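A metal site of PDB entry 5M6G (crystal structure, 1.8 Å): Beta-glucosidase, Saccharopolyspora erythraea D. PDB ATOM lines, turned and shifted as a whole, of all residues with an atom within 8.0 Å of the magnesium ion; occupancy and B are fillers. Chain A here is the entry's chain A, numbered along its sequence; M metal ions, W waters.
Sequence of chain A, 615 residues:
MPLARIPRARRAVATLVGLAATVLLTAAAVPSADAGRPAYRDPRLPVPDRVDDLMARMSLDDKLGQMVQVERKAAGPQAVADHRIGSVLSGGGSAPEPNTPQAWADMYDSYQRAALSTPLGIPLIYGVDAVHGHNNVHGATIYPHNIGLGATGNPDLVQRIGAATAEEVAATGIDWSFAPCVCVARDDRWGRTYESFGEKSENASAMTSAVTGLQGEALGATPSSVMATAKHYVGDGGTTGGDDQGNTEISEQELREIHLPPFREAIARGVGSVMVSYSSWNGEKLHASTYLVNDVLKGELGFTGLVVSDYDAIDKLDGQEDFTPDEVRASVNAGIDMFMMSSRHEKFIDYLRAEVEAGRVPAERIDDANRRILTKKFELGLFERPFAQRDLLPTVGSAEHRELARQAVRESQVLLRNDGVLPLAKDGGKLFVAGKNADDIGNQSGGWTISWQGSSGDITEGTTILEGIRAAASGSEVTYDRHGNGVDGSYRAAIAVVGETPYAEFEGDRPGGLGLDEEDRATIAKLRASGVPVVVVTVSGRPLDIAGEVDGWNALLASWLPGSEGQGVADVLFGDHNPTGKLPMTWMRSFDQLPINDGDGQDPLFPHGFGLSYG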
ATOM      1  N   VAL A 184      18.108 -34.282  20.772  1.00  0.00           N
ATOM      2  CA  VAL A 184      18.020 -32.845  20.516  1.00  0.00           C
ATOM      3  C   VAL A 184      18.482 -32.648  19.077  1.00  0.00           C
ATOM      4  O   VAL A 184      19.687 -32.681  18.793  1.00  0.00           O
ATOM      5  CB  VAL A 184      18.872 -32.050  21.501  1.00  0.00           C
ATOM      6  CG1 VAL A 184      18.803 -30.583  21.198  1.00  0.00           C
ATOM      7  CG2 VAL A 184      18.419 -32.333  22.931  1.00  0.00           C
ATOM      8  N   ALA A 185      17.534 -32.437  18.163  1.00  0.00           N
ATOM      9  CA  ALA A 185      17.852 -32.415  16.737  1.00  0.00           C
ATOM     10  C   ALA A 185      18.395 -31.032  16.369  1.00  0.00           C
ATOM     11  O   ALA A 185      17.664 -30.043  16.400  1.00  0.00           O
ATOM     12  CB  ALA A 185      16.613 -32.750  15.910  1.00  0.00           C
ATOM     13  N   ARG A 186      19.679 -30.990  15.997  1.00  0.00           N
ATOM     14  CA  ARG A 186      20.343 -29.736  15.655  1.00  0.00           C
ATOM     15  C   ARG A 186      20.520 -29.525  14.152  1.00  0.00           C
ATOM     16  O   ARG A 186      20.949 -28.448  13.749  1.00  0.00           O
ATOM     17  CB  ARG A 186      21.728 -29.670  16.320  1.00  0.00           C
ATOM     18  CG  ARG A 186      21.720 -29.973  17.808  1.00  0.00           C
ATOM     19  CD  ARG A 186      21.248 -28.781  18.616  1.00  0.00           C
ATOM     20  NE  ARG A 186      22.221 -27.684  18.599  1.00  0.00           N
ATOM     21  CZ  ARG A 186      21.943 -26.467  19.077  1.00  0.00           C
ATOM     22  NH1 ARG A 186      22.860 -25.501  19.043  1.00  0.00           N
ATOM     23  NH2 ARG A 186      20.746 -26.216  19.588  1.00  0.00           N
ATOM     24  N   ASP A 187      20.216 -30.522  13.322  1.00  0.00           N
ATOM     25  CA  ASP A 187      20.387 -30.396  11.877  1.00  0.00           C
ATOM     26  C   ASP A 187      19.181 -30.985  11.151  1.00  0.00           C
ATOM     27  O   ASP A 187      19.020 -32.215  11.097  1.00  0.00           O
ATOM     28  CB  ASP A 187      21.687 -31.066  11.415  1.00  0.00           C
ATOM     29  CG  ASP A 187      22.096 -30.647  10.015  1.00  0.00           C
ATOM     30  OD1 ASP A 187      21.247 -30.707   9.102  1.00  0.00           O
ATOM     31  OD2 ASP A 187      23.276 -30.271   9.819  1.00  0.00           O
ATOM     32  N   ASP A 188      18.364 -30.121  10.561  1.00  0.00           N
ATOM     33  CA  ASP A 188      17.079 -30.536   9.999  1.00  0.00           C
ATOM     34  C   ASP A 188      17.229 -31.552   8.875  1.00  0.00           C
ATOM     35  O   ASP A 188      16.235 -32.184   8.501  1.00  0.00           O
ATOM     36  CB  ASP A 188      16.308 -29.312   9.500  1.00  0.00           C
ATOM     37  CG  ASP A 188      15.772 -28.463  10.628  1.00  0.00           C
ATOM     38  OD1 ASP A 188      15.826 -28.921  11.794  1.00  0.00           O
ATOM     39  OD2 ASP A 188      15.278 -27.349  10.347  1.00  0.00           O
ATOM     40  N   THR A 193      14.594 -35.930  12.637  1.00  0.00           N
ATOM     41  CA  THR A 193      14.261 -34.638  13.222  1.00  0.00           C
ATOM     42  C   THR A 193      12.864 -34.657  13.828  1.00  0.00           C
ATOM     43  O   THR A 193      12.627 -34.051  14.877  1.00  0.00           O
ATOM     44  CB  THR A 193      14.385 -33.543  12.155  1.00  0.00           C
ATOM     45  OG1 THR A 193      15.753 -33.451  11.736  1.00  0.00           O
ATOM     46  CG2 THR A 193      13.937 -32.189  12.716  1.00  0.00           C
ATOM     47  N   GLY A 198      12.662 -31.001  20.026  1.00  0.00           N
ATOM     48  CA  GLY A 198      13.097 -29.674  19.653  1.00  0.00           C
ATOM     49  C   GLY A 198      14.598 -29.572  19.637  1.00  0.00           C
ATOM     50  O   GLY A 198      15.320 -30.464  20.071  1.00  0.00           O
ATOM     51  N   GLU A 199      15.079 -28.431  19.132  1.00  0.00           N
ATOM     52  CA  GLU A 199      16.500 -28.205  18.977  1.00  0.00           C
ATOM     53  C   GLU A 199      17.181 -27.751  20.259  1.00  0.00           C
ATOM     54  O   GLU A 199      18.420 -27.725  20.309  1.00  0.00           O
ATOM     55  CB  GLU A 199      16.759 -27.168  17.878  1.00  0.00           C
ATOM     56  CG  GLU A 199      16.461 -25.757  18.326  1.00  0.00           C
ATOM     57  CD  GLU A 199      16.573 -24.736  17.189  1.00  0.00           C
ATOM     58  OE1 GLU A 199      16.571 -25.156  16.010  1.00  0.00           O
ATOM     59  OE2 GLU A 199      16.664 -23.529  17.494  1.00  0.00           O
ATOM     60  N   LYS A 200      16.420 -27.352  21.278  1.00  0.00           N
ATOM     61  CA  LYS A 200      16.992 -26.858  22.515  1.00  0.00           C
ATOM     62  C   LYS A 200      16.851 -27.903  23.609  1.00  0.00           C
ATOM     63  O   LYS A 200      15.795 -28.534  23.735  1.00  0.00           O
ATOM     64  CB  LYS A 200      16.325 -25.553  22.963  1.00  0.00           C
ATOM     65  CG  LYS A 200      16.538 -24.414  21.983  1.00  0.00           C
ATOM     66  CD  LYS A 200      15.833 -23.151  22.441  1.00  0.00           C
ATOM     67  CE  LYS A 200      16.516 -22.526  23.631  1.00  0.00           C
ATOM     68  NZ  LYS A 200      17.477 -21.502  23.189  1.00  0.00           N
ATOM     69  N   PRO A 543      11.146 -28.233   9.596  1.00  0.00           N
ATOM     70  CA  PRO A 543      11.046 -27.088   8.690  1.00  0.00           C
ATOM     71  C   PRO A 543      11.406 -27.503   7.269  1.00  0.00           C
ATOM     72  O   PRO A 543      12.231 -28.385   7.055  1.00  0.00           O
ATOM     73  CB  PRO A 543      12.067 -26.096   9.267  1.00  0.00           C
ATOM     74  CG  PRO A 543      12.179 -26.483  10.733  1.00  0.00           C
ATOM     75  CD  PRO A 543      12.045 -27.989  10.731  1.00  0.00           C
ATOM     76  N   PRO A 584       9.485 -25.285  17.667  1.00  0.00           N
ATOM     77  CA  PRO A 584      10.510 -25.970  18.451  1.00  0.00           C
ATOM     78  C   PRO A 584      11.858 -26.073  17.753  1.00  0.00           C
ATOM     79  O   PRO A 584      12.845 -26.465  18.400  1.00  0.00           O
ATOM     80  CB  PRO A 584       9.897 -27.370  18.652  1.00  0.00           C
ATOM     81  CG  PRO A 584       9.141 -27.586  17.359  1.00  0.00           C
ATOM     82  CD  PRO A 584       8.548 -26.232  17.010  1.00  0.00           C
ATOM     83  N   MET A 585      11.924 -25.784  16.457  1.00  0.00           N
ATOM     84  CA  MET A 585      13.167 -25.674  15.704  1.00  0.00           C
ATOM     85  C   MET A 585      13.200 -24.314  15.032  1.00  0.00           C
ATOM     86  O   MET A 585      12.156 -23.769  14.662  1.00  0.00           O
ATOM     87  CB  MET A 585      13.312 -26.767  14.608  1.00  0.00           C
ATOM     88  CG  MET A 585      13.775 -28.171  15.073  1.00  0.00           C
ATOM     89  SD  MET A 585      12.545 -28.978  16.104  1.00  0.00           S
ATOM     90  CE  MET A 585      13.086 -30.691  16.170  1.00  0.00           C
ATOM     91  N   THR A 586      14.398 -23.765  14.878  1.00  0.00           N
ATOM     92  CA  THR A 586      14.583 -22.541  14.114  1.00  0.00           C
ATOM     93  C   THR A 586      14.352 -22.818  12.618  1.00  0.00           C
ATOM     94  O   THR A 586      14.849 -23.811  12.077  1.00  0.00           O
ATOM     95  CB  THR A 586      15.994 -21.994  14.348  1.00  0.00           C
ATOM     96  OG1 THR A 586      16.138 -21.621  15.717  1.00  0.00           O
ATOM     97  CG2 THR A 586      16.254 -20.787  13.488  1.00  0.00           C
ATOM     98  N   TRP A 587      13.605 -21.949  11.953  1.00  0.00           N
ATOM     99  CA  TRP A 587      13.188 -22.188  10.567  1.00  0.00           C
ATOM    100  C   TRP A 587      14.103 -21.445   9.601  1.00  0.00           C
ATOM    101  O   TRP A 587      14.176 -20.204   9.633  1.00  0.00           O
ATOM    102  CB  TRP A 587      11.736 -21.759  10.367  1.00  0.00           C
ATOM    103  CG  TRP A 587      11.097 -22.352   9.150  1.00  0.00           C
ATOM    104  CD1 TRP A 587      11.486 -22.187   7.847  1.00  0.00           C
ATOM    105  CD2 TRP A 587       9.945 -23.204   9.117  1.00  0.00           C
ATOM    106  NE1 TRP A 587      10.643 -22.893   7.005  1.00  0.00           N
ATOM    107  CE2 TRP A 587       9.689 -23.529   7.770  1.00  0.00           C
ATOM    108  CE3 TRP A 587       9.099 -23.736  10.108  1.00  0.00           C
ATOM    109  CZ2 TRP A 587       8.637 -24.350   7.374  1.00  0.00           C
ATOM    110  CZ3 TRP A 587       8.046 -24.556   9.712  1.00  0.00           C
ATOM    111  CH2 TRP A 587       7.825 -24.857   8.363  1.00  0.00           C
ATOM    112  N   MET A 588      14.746 -22.191   8.699  1.00  0.00           N
ATOM    113  CA  MET A 588      15.799 -21.655   7.843  1.00  0.00           C
ATOM    114  C   MET A 588      15.269 -20.611   6.843  1.00  0.00           C
ATOM    115  O   MET A 588      14.150 -20.718   6.321  1.00  0.00           O
ATOM    116  CB  MET A 588      16.456 -22.797   7.066  1.00  0.00           C
ATOM    117  CG  MET A 588      15.557 -23.368   5.956  1.00  0.00           C
ATOM    118  SD  MET A 588      16.054 -24.948   5.274  1.00  0.00           S
ATOM    119  CE  MET A 588      15.046 -26.070   6.251  1.00  0.00           C
ATOM    120  N   LEU A 594      21.758 -24.608   7.213  1.00  0.00           N
ATOM    121  CA  LEU A 594      21.768 -25.792   8.064  1.00  0.00           C
ATOM    122  C   LEU A 594      23.213 -26.185   8.384  1.00  0.00           C
ATOM    123  O   LEU A 594      24.080 -26.134   7.509  1.00  0.00           O
ATOM    124  CB  LEU A 594      21.032 -26.959   7.402  1.00  0.00           C
ATOM    125  CG  LEU A 594      19.597 -26.661   7.007  1.00  0.00           C
ATOM    126  CD1 LEU A 594      18.927 -27.959   6.579  1.00  0.00           C
ATOM    127  CD2 LEU A 594      18.866 -26.009   8.169  1.00  0.00           C
ATOM    128  N   PRO A 595      23.484 -26.572   9.640  1.00  0.00           N
ATOM    129  CA  PRO A 595      22.520 -26.573  10.765  1.00  0.00           C
ATOM    130  C   PRO A 595      22.238 -25.163  11.290  1.00  0.00           C
ATOM    131  O   PRO A 595      23.178 -24.370  11.428  1.00  0.00           O
ATOM    132  CB  PRO A 595      23.235 -27.406  11.826  1.00  0.00           C
ATOM    133  CG  PRO A 595      24.702 -27.147  11.549  1.00  0.00           C
ATOM    134  CD  PRO A 595      24.802 -27.096  10.051  1.00  0.00           C
ATOM    135  N   ILE A 596      20.967 -24.844  11.574  1.00  0.00           N
ATOM    136  CA  ILE A 596      20.611 -23.546  12.136  1.00  0.00           C
ATOM    137  C   ILE A 596      19.925 -23.768  13.482  1.00  0.00           C
ATOM    138  O   ILE A 596      19.030 -24.610  13.597  1.00  0.00           O
ATOM    139  CB  ILE A 596      19.731 -22.716  11.178  1.00  0.00           C
ATOM    140  CG1 ILE A 596      19.488 -21.319  11.769  1.00  0.00           C
ATOM    141  CG2 ILE A 596      18.419 -23.448  10.840  1.00  0.00           C
ATOM    142  CD1 ILE A 596      18.956 -20.310  10.765  1.00  0.00           C
ATOM    143  N   ASN A 597      20.371 -23.036  14.490  1.00  0.00           N
ATOM    144  CA  ASN A 597      19.858 -23.242  15.835  1.00  0.00           C
ATOM    145  C   ASN A 597      19.841 -21.928  16.579  1.00  0.00           C
ATOM    146  O   ASN A 597      20.669 -21.040  16.335  1.00  0.00           O
ATOM    147  CB  ASN A 597      20.696 -24.265  16.602  1.00  0.00           C
ATOM    148  CG  ASN A 597      20.623 -25.637  15.979  1.00  0.00           C
ATOM    149  OD1 ASN A 597      19.645 -26.345  16.172  1.00  0.00           O
ATOM    150  ND2 ASN A 597      21.651 -26.006  15.230  1.00  0.00           N
ATOM    151  N   ASP A 598      18.896 -21.816  17.495  1.00  0.00           N
ATOM    152  CA  ASP A 598      18.725 -20.631  18.320  1.00  0.00           C
ATOM    153  C   ASP A 598      20.052 -20.219  18.944  1.00  0.00           C
ATOM    154  O   ASP A 598      20.773 -21.050  19.509  1.00  0.00           O
ATOM    155  CB  ASP A 598      17.691 -20.913  19.410  1.00  0.00           C
ATOM    156  CG  ASP A 598      17.132 -19.656  20.024  1.00  0.00           C
ATOM    157  OD1 ASP A 598      16.837 -18.710  19.271  1.00  0.00           O
ATOM    158  OD2 ASP A 598      16.992 -19.604  21.265  1.00  0.00           O
ATOM    159  N   ASP A 600      22.770 -19.140  17.339  1.00  0.00           N
ATOM    160  CA  ASP A 600      23.968 -19.313  16.538  1.00  0.00           C
ATOM    161  C   ASP A 600      24.300 -18.084  15.689  1.00  0.00           C
ATOM    162  O   ASP A 600      25.233 -18.155  14.878  1.00  0.00           O
ATOM    163  CB  ASP A 600      23.862 -20.556  15.645  1.00  0.00           C
ATOM    164  CG  ASP A 600      22.854 -20.394  14.502  1.00  0.00           C
ATOM    165  OD1 ASP A 600      22.240 -19.308  14.341  1.00  0.00           O
ATOM    166  OD2 ASP A 600      22.690 -21.397  13.755  1.00  0.00           O
ATOM    167  N   HIS A 608      13.167 -19.741  16.713  1.00  0.00           N
ATOM    168  CA  HIS A 608      12.675 -20.641  17.746  1.00  0.00           C
ATOM    169  C   HIS A 608      11.691 -19.905  18.650  1.00  0.00           C
ATOM    170  O   HIS A 608      11.905 -18.755  19.014  1.00  0.00           O
ATOM    171  CB  HIS A 608      13.873 -21.164  18.555  1.00  0.00           C
ATOM    172  CG  HIS A 608      13.510 -22.212  19.555  1.00  0.00           C
ATOM    173  ND1 HIS A 608      12.908 -21.919  20.765  1.00  0.00           N
ATOM    174  CD2 HIS A 608      13.654 -23.561  19.521  1.00  0.00           C
ATOM    175  CE1 HIS A 608      12.691 -23.046  21.430  1.00  0.00           C
ATOM    176  NE2 HIS A 608      13.147 -24.050  20.703  1.00  0.00           N
HETATM  177 MG    MG M   1      17.770 -26.267  14.609  1.00  0.00          MG
HETATM  178  O   HOH W   1      16.374 -25.955  12.822  1.00  0.00           O
HETATM  179  O   HOH W   2      19.171 -27.191  11.691  1.00  0.00           O
HETATM  180  O   HOH W   3      17.402 -28.438  14.423  1.00  0.00           O
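NH2 of Arg 186 sits at hydrogen-bond distance from O of Glu 199 (2.9 Å).
The side-chain amide nitrogen (ND2) of Asn 597 sits at hydrogen-bond distance from the backbone carbonyl oxygen (O) of Arg 186 (2.9 Å).
N of Glu 199 sits at hydrogen-bond distance from O of Pro 584 (3.1 Å).
OE2 of Glu 199 is in hydrogen-bond range of N of Asp 598, 2.8 Å away.
OG1 of Thr 586 lies within hydrogen-bond range of OE2 of Glu 199 (2.7 Å).
The backbone NH (N) of Asn 597 is in hydrogen-bond range of the side-chain carboxylate (OD2) of Asp 600, 2.9 Å away.
Arg 186 touches the magnesium ion (O to MG, 3.9 Å).
The nearest printed residue that does not touch the magnesium ion is Ala 185 (4.2 Å).
OE1 of Glu 199 binds the magnesium ion, 2.2 Å away.
The magnesium ion is bound by water W3 (2.2 Å).
Water W1 is bound to the magnesium ion, at 2.3 Å.
The backbone carbonyl oxygen (O) of Ile 596 binds the magnesium ion (2.3 Å).
The magnesium ion is bound by the side-chain amide oxygen (OD1) of Asn 597, at 2.4 Å.
The magnesium ion has five donor atoms within binding distance.
Water W3 lies within hydrogen-bond range of the backbone carbonyl oxygen (O) of Ala 185 and the side-chain carboxylate (OD1) of Asp 188.
Water W1 lies within hydrogen-bond range of the backbone carbonyl oxygen of Thr 586 and the side-chain carboxylate of Asp 188.
Water W2 lies within hydrogen-bond range of N of Ile 596, O of Arg 186 and N of Asp 188.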
